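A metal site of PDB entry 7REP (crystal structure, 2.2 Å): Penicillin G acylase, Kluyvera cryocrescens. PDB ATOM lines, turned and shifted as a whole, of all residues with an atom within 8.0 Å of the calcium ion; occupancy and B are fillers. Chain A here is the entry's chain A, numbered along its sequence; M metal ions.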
ATOM      1  N   GLY A  72     -32.266  -0.934  13.367  1.00  0.00           N
ATOM      2  CA  GLY A  72     -30.892  -1.421  13.313  1.00  0.00           C
ATOM      3  C   GLY A  72     -30.643  -2.597  14.236  1.00  0.00           C
ATOM      4  O   GLY A  72     -31.535  -3.011  14.982  1.00  0.00           O
ATOM      5  N   ASP A  73     -29.423  -3.184  14.184  1.00  0.00           N
ATOM      6  CA  ASP A  73     -29.080  -4.309  15.064  1.00  0.00           C
ATOM      7  C   ASP A  73     -28.277  -3.835  16.258  1.00  0.00           C
ATOM      8  O   ASP A  73     -27.047  -3.758  16.226  1.00  0.00           O
ATOM      9  CB  ASP A  73     -28.321  -5.438  14.333  1.00  0.00           C
ATOM     10  CG  ASP A  73     -28.175  -6.727  15.152  1.00  0.00           C
ATOM     11  OD1 ASP A  73     -28.549  -6.727  16.343  1.00  0.00           O
ATOM     12  OD2 ASP A  73     -27.730  -7.742  14.588  1.00  0.00           O
ATOM     13  N   ASP A  74     -28.980  -3.575  17.332  1.00  0.00           N
ATOM     14  CA  ASP A  74     -28.359  -3.148  18.578  1.00  0.00           C
ATOM     15  C   ASP A  74     -28.544  -4.189  19.693  1.00  0.00           C
ATOM     16  O   ASP A  74     -28.357  -3.855  20.860  1.00  0.00           O
ATOM     17  CB  ASP A  74     -28.931  -1.786  18.985  1.00  0.00           C
ATOM     18  CG  ASP A  74     -30.443  -1.760  19.200  1.00  0.00           C
ATOM     19  OD1 ASP A  74     -31.104  -2.761  18.868  1.00  0.00           O
ATOM     20  OD2 ASP A  74     -30.954  -0.732  19.711  1.00  0.00           O
ATOM     21  N   VAL A  75     -28.948  -5.439  19.357  1.00  0.00           N
ATOM     22  CA  VAL A  75     -29.144  -6.513  20.327  1.00  0.00           C
ATOM     23  C   VAL A  75     -28.443  -7.778  19.848  1.00  0.00           C
ATOM     24  O   VAL A  75     -28.668  -8.240  18.720  1.00  0.00           O
ATOM     25  CB  VAL A  75     -30.626  -6.801  20.641  1.00  0.00           C
ATOM     26  CG1 VAL A  75     -30.724  -7.953  21.633  1.00  0.00           C
ATOM     27  CG2 VAL A  75     -31.349  -5.565  21.179  1.00  0.00           C
ATOM     28  N   ASP A  76     -27.574  -8.348  20.704  1.00  0.00           N
ATOM     29  CA  ASP A  76     -26.891  -9.585  20.392  1.00  0.00           C
ATOM     30  C   ASP A  76     -27.160 -10.578  21.491  1.00  0.00           C
ATOM     31  O   ASP A  76     -27.453 -10.193  22.621  1.00  0.00           O
ATOM     32  CB  ASP A  76     -25.392  -9.373  20.209  1.00  0.00           C
ATOM     33  CG  ASP A  76     -24.979  -8.738  18.890  1.00  0.00           C
ATOM     34  OD1 ASP A  76     -25.845  -8.532  18.039  1.00  0.00           O
ATOM     35  OD2 ASP A  76     -23.774  -8.463  18.723  1.00  0.00           O
ATOM     36  N   ILE A  77     -27.107 -11.877  21.174  1.00  0.00           N
ATOM     37  CA  ILE A  77     -27.384 -12.907  22.168  1.00  0.00           C
ATOM     38  C   ILE A  77     -26.082 -13.590  22.501  1.00  0.00           C
ATOM     39  O   ILE A  77     -25.326 -13.952  21.612  1.00  0.00           O
ATOM     40  CB  ILE A  77     -28.459 -13.923  21.704  1.00  0.00           C
ATOM     41  CG1 ILE A  77     -29.758 -13.201  21.304  1.00  0.00           C
ATOM     42  CG2 ILE A  77     -28.734 -14.977  22.806  1.00  0.00           C
ATOM     43  CD1 ILE A  77     -30.455 -12.484  22.434  1.00  0.00           C
ATOM     44  N   ALA A 140     -27.953  -9.056  25.200  1.00  0.00           N
ATOM     45  CA  ALA A 140     -27.104  -7.882  25.281  1.00  0.00           C
ATOM     46  C   ALA A 140     -27.608  -6.737  24.419  1.00  0.00           C
ATOM     47  O   ALA A 140     -27.533  -6.819  23.197  1.00  0.00           O
ATOM     48  CB  ALA A 140     -25.670  -8.231  24.883  1.00  0.00           C
ATOM     49  N   PRO A 197     -23.023  -1.827  18.758  1.00  0.00           N
ATOM     50  CA  PRO A 197     -21.784  -2.468  19.214  1.00  0.00           C
ATOM     51  C   PRO A 197     -20.697  -2.551  18.174  1.00  0.00           C
ATOM     52  O   PRO A 197     -20.959  -2.683  16.979  1.00  0.00           O
ATOM     53  CB  PRO A 197     -22.242  -3.856  19.625  1.00  0.00           C
ATOM     54  CG  PRO A 197     -23.447  -4.117  18.811  1.00  0.00           C
ATOM     55  CD  PRO A 197     -24.114  -2.809  18.583  1.00  0.00           C
ATOM     56  N   ARG A 199     -18.170  -4.881  17.130  1.00  0.00           N
ATOM     57  CA  ARG A 199     -18.056  -6.326  17.264  1.00  0.00           C
ATOM     58  C   ARG A 199     -16.727  -6.863  16.793  1.00  0.00           C
ATOM     59  O   ARG A 199     -16.122  -6.310  15.869  1.00  0.00           O
ATOM     60  CB  ARG A 199     -19.193  -7.000  16.474  1.00  0.00           C
ATOM     61  CG  ARG A 199     -20.598  -6.464  16.771  1.00  0.00           C
ATOM     62  CD  ARG A 199     -21.614  -7.206  15.930  1.00  0.00           C
ATOM     63  NE  ARG A 199     -22.973  -7.079  16.445  1.00  0.00           N
ATOM     64  CZ  ARG A 199     -23.843  -6.154  16.048  1.00  0.00           C
ATOM     65  NH1 ARG A 199     -23.512  -5.270  15.112  1.00  0.00           N
ATOM     66  NH2 ARG A 199     -25.065  -6.123  16.568  1.00  0.00           N
ATOM     67  N   HIS A 203     -17.910 -11.657  13.636  1.00  0.00           N
ATOM     68  CA  HIS A 203     -19.081 -11.787  14.495  1.00  0.00           C
ATOM     69  C   HIS A 203     -20.268 -11.594  13.534  1.00  0.00           C
ATOM     70  O   HIS A 203     -20.418 -10.519  12.962  1.00  0.00           O
ATOM     71  CB  HIS A 203     -19.100 -10.698  15.593  1.00  0.00           C
ATOM     72  CG  HIS A 203     -20.268 -10.747  16.534  1.00  0.00           C
ATOM     73  ND1 HIS A 203     -20.156 -10.314  17.841  1.00  0.00           N
ATOM     74  CD2 HIS A 203     -21.548 -11.170  16.325  1.00  0.00           C
ATOM     75  CE1 HIS A 203     -21.353 -10.486  18.385  1.00  0.00           C
ATOM     76  NE2 HIS A 203     -22.226 -10.994  17.508  1.00  0.00           N
ATOM     77  N   ASP A 204     -21.028 -12.671  13.284  1.00  0.00           N
ATOM     78  CA  ASP A 204     -22.217 -12.593  12.439  1.00  0.00           C
ATOM     79  C   ASP A 204     -23.289 -12.093  13.377  1.00  0.00           C
ATOM     80  O   ASP A 204     -23.651 -12.789  14.330  1.00  0.00           O
ATOM     81  CB  ASP A 204     -22.617 -13.984  11.943  1.00  0.00           C
ATOM     82  CG  ASP A 204     -23.701 -13.965  10.889  1.00  0.00           C
ATOM     83  OD1 ASP A 204     -24.560 -13.044  10.926  1.00  0.00           O
ATOM     84  OD2 ASP A 204     -23.695 -14.842  10.021  1.00  0.00           O
ATOM     85  N   PRO A 205     -23.779 -10.859  13.163  1.00  0.00           N
ATOM     86  CA  PRO A 205     -24.765 -10.284  14.111  1.00  0.00           C
ATOM     87  C   PRO A 205     -26.171 -10.894  14.054  1.00  0.00           C
ATOM     88  O   PRO A 205     -26.998 -10.563  14.916  1.00  0.00           O
ATOM     89  CB  PRO A 205     -24.759  -8.797  13.778  1.00  0.00           C
ATOM     90  CG  PRO A 205     -24.278  -8.706  12.395  1.00  0.00           C
ATOM     91  CD  PRO A 205     -23.445  -9.915  12.082  1.00  0.00           C
ATOM     92  N   ARG A 206     -26.421 -11.815  13.105  1.00  0.00           N
ATOM     93  CA  ARG A 206     -27.706 -12.520  12.974  1.00  0.00           C
ATOM     94  C   ARG A 206     -27.811 -13.767  13.833  1.00  0.00           C
ATOM     95  O   ARG A 206     -28.892 -14.331  13.941  1.00  0.00           O
ATOM     96  CB  ARG A 206     -27.946 -12.920  11.510  1.00  0.00           C
ATOM     97  CG  ARG A 206     -27.897 -11.735  10.558  1.00  0.00           C
ATOM     98  CD  ARG A 206     -27.747 -12.190   9.130  1.00  0.00           C
ATOM     99  NE  ARG A 206     -26.592 -13.057   8.949  1.00  0.00           N
ATOM    100  CZ  ARG A 206     -26.274 -13.672   7.819  1.00  0.00           C
ATOM    101  NH1 ARG A 206     -27.063 -13.556   6.758  1.00  0.00           N
ATOM    102  NH2 ARG A 206     -25.197 -14.435   7.740  1.00  0.00           N
ATOM    103  N   LEU A 207     -26.691 -14.256  14.400  1.00  0.00           N
ATOM    104  CA  LEU A 207     -26.703 -15.507  15.168  1.00  0.00           C
ATOM    105  C   LEU A 207     -26.047 -15.324  16.523  1.00  0.00           C
ATOM    106  O   LEU A 207     -25.193 -14.442  16.679  1.00  0.00           O
ATOM    107  CB  LEU A 207     -25.974 -16.606  14.353  1.00  0.00           C
ATOM    108  CG  LEU A 207     -26.604 -16.887  12.984  1.00  0.00           C
ATOM    109  CD1 LEU A 207     -25.559 -17.273  11.931  1.00  0.00           C
ATOM    110  CD2 LEU A 207     -27.749 -17.879  13.096  1.00  0.00           C
ATOM    111  N   PRO A 208     -26.395 -16.157  17.528  1.00  0.00           N
ATOM    112  CA  PRO A 208     -25.761 -16.011  18.840  1.00  0.00           C
ATOM    113  C   PRO A 208     -24.253 -16.183  18.821  1.00  0.00           C
ATOM    114  O   PRO A 208     -23.696 -16.783  17.901  1.00  0.00           O
ATOM    115  CB  PRO A 208     -26.439 -17.095  19.705  1.00  0.00           C
ATOM    116  CG  PRO A 208     -27.722 -17.422  18.982  1.00  0.00           C
ATOM    117  CD  PRO A 208     -27.385 -17.246  17.512  1.00  0.00           C
ATOM    118  N   TRP A 217     -18.101  -7.743  22.936  1.00  0.00           N
ATOM    119  CA  TRP A 217     -17.962  -6.557  22.086  1.00  0.00           C
ATOM    120  C   TRP A 217     -16.709  -5.774  22.463  1.00  0.00           C
ATOM    121  O   TRP A 217     -16.397  -5.658  23.651  1.00  0.00           O
ATOM    122  CB  TRP A 217     -19.172  -5.622  22.261  1.00  0.00           C
ATOM    123  CG  TRP A 217     -20.506  -6.160  21.831  1.00  0.00           C
ATOM    124  CD1 TRP A 217     -20.763  -7.054  20.825  1.00  0.00           C
ATOM    125  CD2 TRP A 217     -21.780  -5.769  22.360  1.00  0.00           C
ATOM    126  NE1 TRP A 217     -22.118  -7.262  20.721  1.00  0.00           N
ATOM    127  CE2 TRP A 217     -22.768  -6.473  21.632  1.00  0.00           C
ATOM    128  CE3 TRP A 217     -22.186  -4.831  23.306  1.00  0.00           C
ATOM    129  CZ2 TRP A 217     -24.127  -6.281  21.872  1.00  0.00           C
ATOM    130  CZ3 TRP A 217     -23.529  -4.682  23.569  1.00  0.00           C
ATOM    131  CH2 TRP A 217     -24.486  -5.395  22.847  1.00  0.00           C
ATOM    132  N   ALA A 250     -29.619  -4.260   8.887  1.00  0.00           N
ATOM    133  CA  ALA A 250     -30.870  -4.285   9.606  1.00  0.00           C
ATOM    134  C   ALA A 250     -30.741  -5.127  10.866  1.00  0.00           C
ATOM    135  O   ALA A 250     -29.794  -5.903  11.000  1.00  0.00           O
ATOM    136  CB  ALA A 250     -31.973  -4.861   8.693  1.00  0.00           C
ATOM    137  N   SER A 251     -31.723  -5.011  11.768  1.00  0.00           N
ATOM    138  CA  SER A 251     -31.976  -5.840  12.936  1.00  0.00           C
ATOM    139  C   SER A 251     -31.899  -7.328  12.522  1.00  0.00           C
ATOM    140  O   SER A 251     -32.186  -7.658  11.366  1.00  0.00           O
ATOM    141  CB  SER A 251     -33.387  -5.553  13.435  1.00  0.00           C
ATOM    142  OG  SER A 251     -33.865  -6.496  14.379  1.00  0.00           O
ATOM    143  N   ASP A 252     -31.500  -8.191  13.429  1.00  0.00           N
ATOM    144  CA  ASP A 252     -31.369  -9.617  13.108  1.00  0.00           C
ATOM    145  C   ASP A 252     -32.753 -10.361  13.083  1.00  0.00           C
ATOM    146  O   ASP A 252     -32.771 -11.561  12.826  1.00  0.00           O
ATOM    147  CB  ASP A 252     -30.384 -10.276  14.073  1.00  0.00           C
ATOM    148  CG  ASP A 252     -30.927 -10.303  15.481  1.00  0.00           C
ATOM    149  OD1 ASP A 252     -31.975 -10.929  15.690  1.00  0.00           O
ATOM    150  OD2 ASP A 252     -30.310  -9.699  16.375  1.00  0.00           O
ATOM    151  N   SER A 253     -33.886  -9.680  13.381  1.00  0.00           N
ATOM    152  CA  SER A 253     -35.204 -10.341  13.359  1.00  0.00           C
ATOM    153  C   SER A 253     -35.514 -10.918  11.993  1.00  0.00           C
ATOM    154  O   SER A 253     -35.439 -10.183  11.013  1.00  0.00           O
ATOM    155  CB  SER A 253     -36.294  -9.371  13.780  1.00  0.00           C
ATOM    156  OG  SER A 253     -36.432  -9.447  15.181  1.00  0.00           O
ATOM    157  N   SER A 704     -35.425  -5.644  19.691  1.00  0.00           N
ATOM    158  CA  SER A 704     -35.821  -6.739  18.786  1.00  0.00           C
ATOM    159  C   SER A 704     -34.695  -7.624  18.271  1.00  0.00           C
ATOM    160  O   SER A 704     -33.758  -7.186  17.594  1.00  0.00           O
ATOM    161  CB  SER A 704     -36.663  -6.230  17.626  1.00  0.00           C
ATOM    162  OG  SER A 704     -35.898  -5.423  16.759  1.00  0.00           O
ATOM    163  N   THR A 705     -34.814  -8.897  18.622  1.00  0.00           N
ATOM    164  CA  THR A 705     -33.884  -9.913  18.181  1.00  0.00           C
ATOM    165  C   THR A 705     -34.600 -11.250  18.007  1.00  0.00           C
ATOM    166  O   THR A 705     -35.551 -11.564  18.731  1.00  0.00           O
ATOM    167  CB  THR A 705     -32.681 -10.027  19.152  1.00  0.00           C
ATOM    168  OG1 THR A 705     -31.669 -10.836  18.546  1.00  0.00           O
ATOM    169  CG2 THR A 705     -33.065 -10.612  20.494  1.00  0.00           C
ATOM    170  N   SER A 706     -34.123 -12.044  17.072  1.00  0.00           N
ATOM    171  CA  SER A 706     -34.607 -13.408  16.881  1.00  0.00           C
ATOM    172  C   SER A 706     -33.404 -14.344  16.635  1.00  0.00           C
ATOM    173  O   SER A 706     -33.550 -15.309  15.913  1.00  0.00           O
ATOM    174  CB  SER A 706     -35.596 -13.479  15.705  1.00  0.00           C
ATOM    175  OG  SER A 706     -34.938 -13.455  14.447  1.00  0.00           O
ATOM    176  N   GLU A 707     -32.219 -14.058  17.242  1.00  0.00           N
ATOM    177  CA  GLU A 707     -31.002 -14.836  17.025  1.00  0.00           C
ATOM    178  C   GLU A 707     -31.131 -16.326  17.340  1.00  0.00           C
ATOM    179  O   GLU A 707     -30.587 -17.120  16.580  1.00  0.00           O
ATOM    180  CB  GLU A 707     -29.796 -14.232  17.759  1.00  0.00           C
ATOM    181  CG  GLU A 707     -29.284 -12.968  17.084  1.00  0.00           C
ATOM    182  CD  GLU A 707     -28.109 -12.277  17.752  1.00  0.00           C
ATOM    183  OE1 GLU A 707     -27.448 -12.927  18.598  1.00  0.00           O
ATOM    184  OE2 GLU A 707     -27.831 -11.100  17.424  1.00  0.00           O
ATOM    185  N   ASN A 710     -33.163 -17.764  14.590  1.00  0.00           N
ATOM    186  CA  ASN A 710     -32.264 -17.741  13.440  1.00  0.00           C
ATOM    187  C   ASN A 710     -31.311 -18.937  13.462  1.00  0.00           C
ATOM    188  O   ASN A 710     -31.086 -19.549  12.422  1.00  0.00           O
ATOM    189  CB  ASN A 710     -31.462 -16.455  13.418  1.00  0.00           C
ATOM    190  CG  ASN A 710     -32.293 -15.244  13.083  1.00  0.00           C
ATOM    191  OD1 ASN A 710     -33.491 -15.311  12.809  1.00  0.00           O
ATOM    192  ND2 ASN A 710     -31.647 -14.096  13.130  1.00  0.00           N
ATOM    193  N   LEU A 736     -27.602 -10.216   5.371  1.00  0.00           N
ATOM    194  CA  LEU A 736     -27.115  -9.213   6.327  1.00  0.00           C
ATOM    195  C   LEU A 736     -27.346  -7.829   5.751  1.00  0.00           C
ATOM    196  O   LEU A 736     -27.873  -6.943   6.429  1.00  0.00           O
ATOM    197  CB  LEU A 736     -25.639  -9.446   6.688  1.00  0.00           C
ATOM    198  CG  LEU A 736     -25.110  -8.622   7.871  1.00  0.00           C
ATOM    199  CD1 LEU A 736     -25.960  -8.796   9.119  1.00  0.00           C
ATOM    200  CD2 LEU A 736     -23.713  -9.049   8.216  1.00  0.00           C
HETATM  201 CA    CA M   1     -27.911  -9.015  16.565  1.00  0.00          CA
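The calcium ion is bound by the side-chain carboxylate (OE2) of Glu 707 (2.3 Å), the side-chain carboxylate (OD2) of Asp 73 (2.4 Å), the side-chain carboxylate (OD1) of Asp 73 (2.4 Å), the backbone carbonyl oxygen (O) of Val 75 (2.4 Å), the backbone carbonyl oxygen (O) of Pro 205 (2.4 Å), the side-chain carboxylate (OD2) of Asp 252 (2.5 Å) and the side-chain carboxylate (OD1) of Asp 76 (2.6 Å).
The calcium ion has seven donor atoms within binding distance.
The backbone NH (N) of Ile 77 lies within hydrogen-bond range of the side-chain carboxylate (OE1) of Glu 707, 2.8 Å away.
The backbone carbonyl oxygen (O) of Asp 73 is in hydrogen-bond range of the guanidinium group (NH2) of Arg 199.
The backbone NH (N) of Ser 706 is in hydrogen-bond range of the side-chain carboxylate (OD1) of Asp 252.
The backbone carbonyl oxygen (O) of Asp 252 sits at hydrogen-bond distance from the side-chain amide nitrogen (ND2) of Asn 710 (2.8 Å).
OD2 of Asp 76 is in salt-bridge range of NE of Arg 199 (2.8 Å).
NE2 of His 203 sits close to OD2 of Asp 76 (3.2 Å).
The backbone NH (N) of Ala 140 is in hydrogen-bond range of the backbone carbonyl oxygen (O) of Asp 76 (2.9 Å).
NE1 of Trp 217 lies within hydrogen-bond range of OD2 of Asp 76 (2.9 Å).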
